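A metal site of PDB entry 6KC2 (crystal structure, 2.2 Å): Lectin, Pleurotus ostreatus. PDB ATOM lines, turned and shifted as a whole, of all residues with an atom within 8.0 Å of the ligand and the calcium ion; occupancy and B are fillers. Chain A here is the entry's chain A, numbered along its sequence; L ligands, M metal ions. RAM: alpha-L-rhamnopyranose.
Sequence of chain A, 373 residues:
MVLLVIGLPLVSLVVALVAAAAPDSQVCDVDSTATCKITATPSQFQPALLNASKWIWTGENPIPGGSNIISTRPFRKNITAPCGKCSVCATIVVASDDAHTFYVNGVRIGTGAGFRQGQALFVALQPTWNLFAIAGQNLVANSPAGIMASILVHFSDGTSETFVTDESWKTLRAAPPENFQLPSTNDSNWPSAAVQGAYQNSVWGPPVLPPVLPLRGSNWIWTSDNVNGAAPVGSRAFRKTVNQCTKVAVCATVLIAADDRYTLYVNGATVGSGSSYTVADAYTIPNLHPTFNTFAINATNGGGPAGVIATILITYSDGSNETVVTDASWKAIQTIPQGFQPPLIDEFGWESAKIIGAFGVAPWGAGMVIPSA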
ATOM      1  N   TRP A  57      -4.364  -9.794  20.411  1.00  0.00           N
ATOM      2  CA  TRP A  57      -4.245 -11.016  19.639  1.00  0.00           C
ATOM      3  C   TRP A  57      -4.880 -10.726  18.292  1.00  0.00           C
ATOM      4  O   TRP A  57      -4.997  -9.557  17.890  1.00  0.00           O
ATOM      5  CB  TRP A  57      -4.880 -12.203  20.386  1.00  0.00           C
ATOM      6  CG  TRP A  57      -4.418 -13.536  19.855  1.00  0.00           C
ATOM      7  CD1 TRP A  57      -5.193 -14.494  19.265  1.00  0.00           C
ATOM      8  CD2 TRP A  57      -3.073 -14.046  19.851  1.00  0.00           C
ATOM      9  NE1 TRP A  57      -4.421 -15.565  18.906  1.00  0.00           N
ATOM     10  CE2 TRP A  57      -3.115 -15.320  19.244  1.00  0.00           C
ATOM     11  CE3 TRP A  57      -1.836 -13.546  20.294  1.00  0.00           C
ATOM     12  CZ2 TRP A  57      -1.971 -16.122  19.072  1.00  0.00           C
ATOM     13  CZ3 TRP A  57      -0.687 -14.339  20.125  1.00  0.00           C
ATOM     14  CH2 TRP A  57      -0.766 -15.617  19.520  1.00  0.00           C
ATOM     15  N   GLY A  65     -10.003 -12.726  25.558  1.00  0.00           N
ATOM     16  CA  GLY A  65      -9.682 -13.677  26.599  1.00  0.00           C
ATOM     17  C   GLY A  65     -10.294 -15.044  26.376  1.00  0.00           C
ATOM     18  O   GLY A  65     -10.286 -15.877  27.288  1.00  0.00           O
ATOM     19  N   GLY A  66     -10.824 -15.285  25.186  1.00  0.00           N
ATOM     20  CA  GLY A  66     -11.445 -16.544  24.873  1.00  0.00           C
ATOM     21  C   GLY A  66     -10.431 -17.588  24.437  1.00  0.00           C
ATOM     22  O   GLY A  66      -9.238 -17.329  24.277  1.00  0.00           O
ATOM     23  N   SER A  67     -10.941 -18.797  24.226  1.00  0.00           N
ATOM     24  CA  SER A  67     -10.082 -19.901  23.825  1.00  0.00           C
ATOM     25  C   SER A  67      -9.585 -19.686  22.395  1.00  0.00           C
ATOM     26  O   SER A  67     -10.330 -19.226  21.515  1.00  0.00           O
ATOM     27  CB  SER A  67     -10.824 -21.229  23.968  1.00  0.00           C
ATOM     28  OG  SER A  67     -11.441 -21.590  22.772  1.00  0.00           O
ATOM     29  N   ASN A  68      -8.314 -19.995  22.176  1.00  0.00           N
ATOM     30  CA  ASN A  68      -7.663 -19.879  20.877  1.00  0.00           C
ATOM     31  C   ASN A  68      -6.894 -21.157  20.594  1.00  0.00           C
ATOM     32  O   ASN A  68      -6.557 -21.933  21.501  1.00  0.00           O
ATOM     33  CB  ASN A  68      -6.717 -18.683  20.841  1.00  0.00           C
ATOM     34  CG  ASN A  68      -7.482 -17.366  20.692  1.00  0.00           C
ATOM     35  OD1 ASN A  68      -7.962 -16.786  21.682  1.00  0.00           O
ATOM     36  ND2 ASN A  68      -7.607 -16.909  19.465  1.00  0.00           N
ATOM     37  N   ILE A  69      -6.615 -21.367  19.322  1.00  0.00           N
ATOM     38  CA  ILE A  69      -5.870 -22.548  18.881  1.00  0.00           C
ATOM     39  C   ILE A  69      -4.375 -22.332  19.088  1.00  0.00           C
ATOM     40  O   ILE A  69      -3.886 -21.198  19.159  1.00  0.00           O
ATOM     41  CB  ILE A  69      -6.180 -22.855  17.407  1.00  0.00           C
ATOM     42  CG1 ILE A  69      -5.612 -21.722  16.533  1.00  0.00           C
ATOM     43  CG2 ILE A  69      -7.711 -23.020  17.164  1.00  0.00           C
ATOM     44  CD1 ILE A  69      -5.497 -22.100  15.045  1.00  0.00           C
ATOM     45  N   ILE A  70      -3.641 -23.443  19.150  1.00  0.00           N
ATOM     46  CA  ILE A  70      -2.179 -23.379  19.070  1.00  0.00           C
ATOM     47  C   ILE A  70      -1.801 -22.752  17.740  1.00  0.00           C
ATOM     48  O   ILE A  70      -2.288 -23.159  16.673  1.00  0.00           O
ATOM     49  CB  ILE A  70      -1.571 -24.774  19.241  1.00  0.00           C
ATOM     50  CG1 ILE A  70      -1.883 -25.311  20.646  1.00  0.00           C
ATOM     51  CG2 ILE A  70      -0.067 -24.714  19.029  1.00  0.00           C
ATOM     52  CD1 ILE A  70      -1.446 -26.757  20.879  1.00  0.00           C
ATOM     53  N   SER A  96       3.555 -12.115  27.698  1.00  0.00           N
ATOM     54  CA  SER A  96       2.881 -12.889  26.669  1.00  0.00           C
ATOM     55  C   SER A  96       2.184 -14.102  27.252  1.00  0.00           C
ATOM     56  O   SER A  96       2.620 -14.710  28.234  1.00  0.00           O
ATOM     57  CB  SER A  96       3.846 -13.377  25.581  1.00  0.00           C
ATOM     58  OG  SER A  96       4.944 -14.082  26.152  1.00  0.00           O
ATOM     59  N   ASP A  97       1.108 -14.473  26.581  1.00  0.00           N
ATOM     60  CA  ASP A  97       0.460 -15.765  26.770  1.00  0.00           C
ATOM     61  C   ASP A  97       0.403 -16.370  25.376  1.00  0.00           C
ATOM     62  O   ASP A  97      -0.469 -15.977  24.591  1.00  0.00           O
ATOM     63  CB  ASP A  97      -0.928 -15.573  27.381  1.00  0.00           C
ATOM     64  CG  ASP A  97      -1.702 -16.875  27.506  1.00  0.00           C
ATOM     65  OD1 ASP A  97      -1.250 -17.914  26.970  1.00  0.00           O
ATOM     66  OD2 ASP A  97      -2.766 -16.842  28.155  1.00  0.00           O
ATOM     67  N   ASP A  98       1.304 -17.312  25.060  1.00  0.00           N
ATOM     68  CA  ASP A  98       2.254 -17.942  25.993  1.00  0.00           C
ATOM     69  C   ASP A  98       3.723 -17.492  25.847  1.00  0.00           C
ATOM     70  O   ASP A  98       4.486 -17.571  26.800  1.00  0.00           O
ATOM     71  CB  ASP A  98       2.240 -19.477  25.824  1.00  0.00           C
ATOM     72  CG  ASP A  98       0.904 -20.093  26.168  1.00  0.00           C
ATOM     73  OD1 ASP A  98       0.725 -20.451  27.355  1.00  0.00           O
ATOM     74  OD2 ASP A  98       0.057 -20.264  25.246  1.00  0.00           O
ATOM     75  N   ALA A  99       4.133 -17.075  24.640  1.00  0.00           N
ATOM     76  CA  ALA A  99       5.541 -16.810  24.374  1.00  0.00           C
ATOM     77  C   ALA A  99       5.671 -15.738  23.300  1.00  0.00           C
ATOM     78  O   ALA A  99       4.737 -15.519  22.512  1.00  0.00           O
ATOM     79  CB  ALA A  99       6.291 -18.098  23.945  1.00  0.00           C
ATOM     80  N   GLY A 114       5.347 -15.843  29.217  1.00  0.00           N
ATOM     81  CA  GLY A 114       4.694 -15.768  30.511  1.00  0.00           C
ATOM     82  C   GLY A 114       4.023 -14.421  30.728  1.00  0.00           C
ATOM     83  O   GLY A 114       4.521 -13.375  30.283  1.00  0.00           O
ATOM     84  N   PHE A 115       2.906 -14.443  31.431  1.00  0.00           N
ATOM     85  CA  PHE A 115       2.096 -13.244  31.635  1.00  0.00           C
ATOM     86  C   PHE A 115       2.074 -12.775  33.076  1.00  0.00           C
ATOM     87  O   PHE A 115       1.578 -11.668  33.348  1.00  0.00           O
ATOM     88  CB  PHE A 115       0.653 -13.496  31.160  1.00  0.00           C
ATOM     89  CG  PHE A 115      -0.022 -14.650  31.858  1.00  0.00           C
ATOM     90  CD1 PHE A 115      -0.720 -14.444  33.057  1.00  0.00           C
ATOM     91  CD2 PHE A 115       0.034 -15.940  31.324  1.00  0.00           C
ATOM     92  CE1 PHE A 115      -1.356 -15.511  33.704  1.00  0.00           C
ATOM     93  CE2 PHE A 115      -0.583 -17.017  31.967  1.00  0.00           C
ATOM     94  CZ  PHE A 115      -1.271 -16.800  33.157  1.00  0.00           C
ATOM     95  N   ARG A 116       2.594 -13.577  34.020  1.00  0.00           N
ATOM     96  CA  ARG A 116       2.594 -13.174  35.413  1.00  0.00           C
ATOM     97  C   ARG A 116       3.654 -12.124  35.696  1.00  0.00           C
ATOM     98  O   ARG A 116       3.483 -11.290  36.596  1.00  0.00           O
ATOM     99  CB  ARG A 116       2.806 -14.399  36.319  1.00  0.00           C
ATOM    100  CG  ARG A 116       1.736 -15.500  36.164  1.00  0.00           C
ATOM    101  CD  ARG A 116       0.627 -15.395  37.215  1.00  0.00           C
ATOM    102  NE  ARG A 116      -0.359 -16.491  37.104  1.00  0.00           N
ATOM    103  CZ  ARG A 116      -1.685 -16.318  37.142  1.00  0.00           C
ATOM    104  NH1 ARG A 116      -2.200 -15.110  37.296  1.00  0.00           N
ATOM    105  NH2 ARG A 116      -2.493 -17.378  37.020  1.00  0.00           N
ATOM    106  N   GLN A 137       3.028 -16.527  20.394  1.00  0.00           N
ATOM    107  CA  GLN A 137       2.663 -17.931  20.232  1.00  0.00           C
ATOM    108  C   GLN A 137       1.700 -18.346  21.333  1.00  0.00           C
ATOM    109  O   GLN A 137       1.978 -18.127  22.515  1.00  0.00           O
ATOM    110  CB  GLN A 137       3.874 -18.877  20.295  1.00  0.00           C
ATOM    111  CG  GLN A 137       5.049 -18.577  19.392  1.00  0.00           C
ATOM    112  CD  GLN A 137       6.258 -19.453  19.778  1.00  0.00           C
ATOM    113  OE1 GLN A 137       6.137 -20.678  19.869  1.00  0.00           O
ATOM    114  NE2 GLN A 137       7.409 -18.812  20.047  1.00  0.00           N
ATOM    115  N   ASN A 138       0.589 -18.967  20.937  1.00  0.00           N
ATOM    116  CA  ASN A 138      -0.274 -19.684  21.855  1.00  0.00           C
ATOM    117  C   ASN A 138       0.163 -21.156  21.868  1.00  0.00           C
ATOM    118  O   ASN A 138       0.186 -21.796  20.810  1.00  0.00           O
ATOM    119  CB  ASN A 138      -1.728 -19.548  21.446  1.00  0.00           C
ATOM    120  CG  ASN A 138      -2.665 -20.090  22.492  1.00  0.00           C
ATOM    121  OD1 ASN A 138      -2.315 -20.149  23.672  1.00  0.00           O
ATOM    122  ND2 ASN A 138      -3.877 -20.481  22.078  1.00  0.00           N
ATOM    123  N   LEU A 139       0.493 -21.686  23.042  1.00  0.00           N
ATOM    124  CA  LEU A 139       1.089 -23.019  23.118  1.00  0.00           C
ATOM    125  C   LEU A 139       0.171 -24.068  23.735  1.00  0.00           C
ATOM    126  O   LEU A 139       0.536 -25.243  23.763  1.00  0.00           O
ATOM    127  CB  LEU A 139       2.424 -22.971  23.888  1.00  0.00           C
ATOM    128  CG  LEU A 139       3.544 -22.157  23.221  1.00  0.00           C
ATOM    129  CD1 LEU A 139       4.772 -22.032  24.129  1.00  0.00           C
ATOM    130  CD2 LEU A 139       3.950 -22.773  21.878  1.00  0.00           C
ATOM    131  N   VAL A 140      -1.003 -23.679  24.235  1.00  0.00           N
ATOM    132  CA  VAL A 140      -1.942 -24.621  24.834  1.00  0.00           C
ATOM    133  C   VAL A 140      -3.271 -24.499  24.095  1.00  0.00           C
ATOM    134  O   VAL A 140      -3.783 -23.384  23.921  1.00  0.00           O
ATOM    135  CB  VAL A 140      -2.114 -24.365  26.341  1.00  0.00           C
ATOM    136  CG1 VAL A 140      -3.131 -25.309  26.939  1.00  0.00           C
ATOM    137  CG2 VAL A 140      -0.791 -24.504  27.044  1.00  0.00           C
ATOM    138  N   ALA A 141      -3.824 -25.630  23.653  1.00  0.00           N
ATOM    139  CA  ALA A 141      -5.070 -25.591  22.903  1.00  0.00           C
ATOM    140  C   ALA A 141      -6.228 -25.133  23.785  1.00  0.00           C
ATOM    141  O   ALA A 141      -6.230 -25.357  24.994  1.00  0.00           O
ATOM    142  CB  ALA A 141      -5.378 -26.970  22.300  1.00  0.00           C
ATOM    143  N   ASN A 142      -7.215 -24.462  23.172  1.00  0.00           N
ATOM    144  CA  ASN A 142      -8.408 -23.983  23.857  1.00  0.00           C
ATOM    145  C   ASN A 142      -8.104 -22.976  24.967  1.00  0.00           C
ATOM    146  O   ASN A 142      -8.885 -22.848  25.921  1.00  0.00           O
ATOM    147  CB  ASN A 142      -9.223 -25.138  24.464  1.00  0.00           C
ATOM    148  CG  ASN A 142      -9.591 -26.191  23.460  1.00  0.00           C
ATOM    149  OD1 ASN A 142     -10.072 -25.883  22.371  1.00  0.00           O
ATOM    150  ND2 ASN A 142      -9.333 -27.445  23.808  1.00  0.00           N
ATOM    151  N   SER A 143      -6.986 -22.270  24.882  1.00  0.00           N
ATOM    152  CA  SER A 143      -6.553 -21.385  25.956  1.00  0.00           C
ATOM    153  C   SER A 143      -6.447 -19.953  25.448  1.00  0.00           C
ATOM    154  O   SER A 143      -6.334 -19.712  24.247  1.00  0.00           O
ATOM    155  CB  SER A 143      -5.194 -21.836  26.529  1.00  0.00           C
ATOM    156  OG  SER A 143      -4.151 -21.501  25.639  1.00  0.00           O
ATOM    157  N   PRO A 144      -6.476 -18.966  26.348  1.00  0.00           N
ATOM    158  CA  PRO A 144      -6.331 -17.576  25.910  1.00  0.00           C
ATOM    159  C   PRO A 144      -4.980 -17.328  25.255  1.00  0.00           C
ATOM    160  O   PRO A 144      -4.038 -18.109  25.391  1.00  0.00           O
ATOM    161  CB  PRO A 144      -6.492 -16.743  27.195  1.00  0.00           C
ATOM    162  CG  PRO A 144      -6.724 -17.704  28.295  1.00  0.00           C
ATOM    163  CD  PRO A 144      -6.945 -19.083  27.742  1.00  0.00           C
ATOM    164  N   ALA A 145      -4.900 -16.230  24.524  1.00  0.00           N
ATOM    165  CA  ALA A 145      -3.674 -15.857  23.838  1.00  0.00           C
ATOM    166  C   ALA A 145      -3.575 -14.338  23.816  1.00  0.00           C
ATOM    167  O   ALA A 145      -4.581 -13.642  23.623  1.00  0.00           O
ATOM    168  CB  ALA A 145      -3.627 -16.425  22.418  1.00  0.00           C
ATOM    169  N   GLY A 146      -2.365 -13.824  23.986  1.00  0.00           N
ATOM    170  CA  GLY A 146      -2.189 -12.389  24.051  1.00  0.00           C
ATOM    171  C   GLY A 146      -0.773 -11.898  24.219  1.00  0.00           C
ATOM    172  O   GLY A 146       0.082 -12.580  24.810  1.00  0.00           O
ATOM    173  N   VAL A 203      -8.299 -11.439  31.571  1.00  0.00           N
ATOM    174  CA  VAL A 203      -8.226 -12.760  32.179  1.00  0.00           C
ATOM    175  C   VAL A 203      -6.887 -12.964  32.893  1.00  0.00           C
ATOM    176  O   VAL A 203      -6.802 -13.765  33.829  1.00  0.00           O
ATOM    177  CB  VAL A 203      -8.476 -13.873  31.151  1.00  0.00           C
ATOM    178  CG1 VAL A 203      -9.912 -13.817  30.674  1.00  0.00           C
ATOM    179  CG2 VAL A 203      -7.478 -13.798  29.982  1.00  0.00           C
ATOM    180  N   TRP A 204      -5.852 -12.207  32.498  1.00  0.00           N
ATOM    181  CA  TRP A 204      -4.517 -12.430  33.038  1.00  0.00           C
ATOM    182  C   TRP A 204      -4.257 -11.714  34.357  1.00  0.00           C
ATOM    183  O   TRP A 204      -3.415 -12.168  35.125  1.00  0.00           O
ATOM    184  CB  TRP A 204      -3.471 -12.018  32.000  1.00  0.00           C
ATOM    185  CG  TRP A 204      -3.593 -12.863  30.784  1.00  0.00           C
ATOM    186  CD1 TRP A 204      -3.188 -14.185  30.641  1.00  0.00           C
ATOM    187  CD2 TRP A 204      -4.207 -12.493  29.539  1.00  0.00           C
ATOM    188  NE1 TRP A 204      -3.514 -14.637  29.377  1.00  0.00           N
ATOM    189  CE2 TRP A 204      -4.123 -13.619  28.682  1.00  0.00           C
ATOM    190  CE3 TRP A 204      -4.800 -11.310  29.068  1.00  0.00           C
ATOM    191  CZ2 TRP A 204      -4.622 -13.592  27.379  1.00  0.00           C
ATOM    192  CZ3 TRP A 204      -5.291 -11.293  27.780  1.00  0.00           C
ATOM    193  CH2 TRP A 204      -5.195 -12.422  26.941  1.00  0.00           C
HETATM  194  C1  RAM L   1      -2.531 -22.128  31.142  1.00  0.00           C
HETATM  195  C2  RAM L   1      -1.603 -22.090  29.926  1.00  0.00           C
HETATM  196  C3  RAM L   1      -2.344 -21.412  28.774  1.00  0.00           C
HETATM  197  C4  RAM L   1      -2.745 -20.009  29.205  1.00  0.00           C
HETATM  198  C5  RAM L   1      -3.534 -20.060  30.515  1.00  0.00           C
HETATM  199  C6  RAM L   1      -3.820 -18.667  31.041  1.00  0.00           C
HETATM  200  O1  RAM L   1      -3.713 -22.900  30.845  1.00  0.00           O
HETATM  201  O2  RAM L   1      -0.454 -21.327  30.232  1.00  0.00           O
HETATM  202  O3  RAM L   1      -1.499 -21.365  27.648  1.00  0.00           O
HETATM  203  O4  RAM L   1      -3.491 -19.417  28.167  1.00  0.00           O
HETATM  204  O5  RAM L   1      -2.823 -20.777  31.518  1.00  0.00           O
HETATM  205 CA    CA M   1      -2.377 -19.755  25.982  1.00  0.00          CA
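Merely in contact with the ligand: Val 140 and Phe 115.
Hydrophobic or aromatic side chains within 4 Å of the ligand: Phe 115, Val 140 and Pro 144.
Six residues have an atom within 4 Å of the ligand: Asp 97, Asp 98, Phe 115, Val 140, Ser 143 and Pro 144.
The nearest printed residue that does not touch the ligand is Asn 138 (4.2 Å).
The calcium ion is bound by the side-chain amide oxygen (OD1) of Asn 138 (2.3 Å), the side-chain carboxylate (OD1) of Asp 97 (2.4 Å), the backbone carbonyl oxygen (O) of Pro 144 (2.4 Å), an oxygen (O4) of the ligand (2.5 Å), an oxygen (O3) of the ligand (2.5 Å), the side-chain hydroxyl (OG) of Ser 143 (2.5 Å) and the side-chain carboxylate (OD2) of Asp 98 (2.6 Å).
The calcium ion has seven donor atoms within binding distance.
ND2 of Asn 138 sits at hydrogen-bond distance from O of Asn 68, at 3.1 Å.
O of Ile 69 is in hydrogen-bond range of ND2 of Asn 138 (3.0 Å).
O of Gly 146 is in hydrogen-bond range of N of Asp 97, 2.8 Å away.
OD2 of Asp 98 lies close to N of Leu 139 (2.7 Å).
N of Asp 98 is in hydrogen-bond range of O of Gln 137 (2.8 Å).
The backbone NH (N) of Gly 114 lies within hydrogen-bond range of the backbone carbonyl oxygen (O) of Asp 98 (3.1 Å).
The side-chain hydroxyl (OG) of Ser 143 lies close to the backbone carbonyl oxygen (O) of Val 140.
The backbone carbonyl oxygen of Ser 143 is in hydrogen-bond range of the backbone NH of Asn 68 (2.9 Å).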
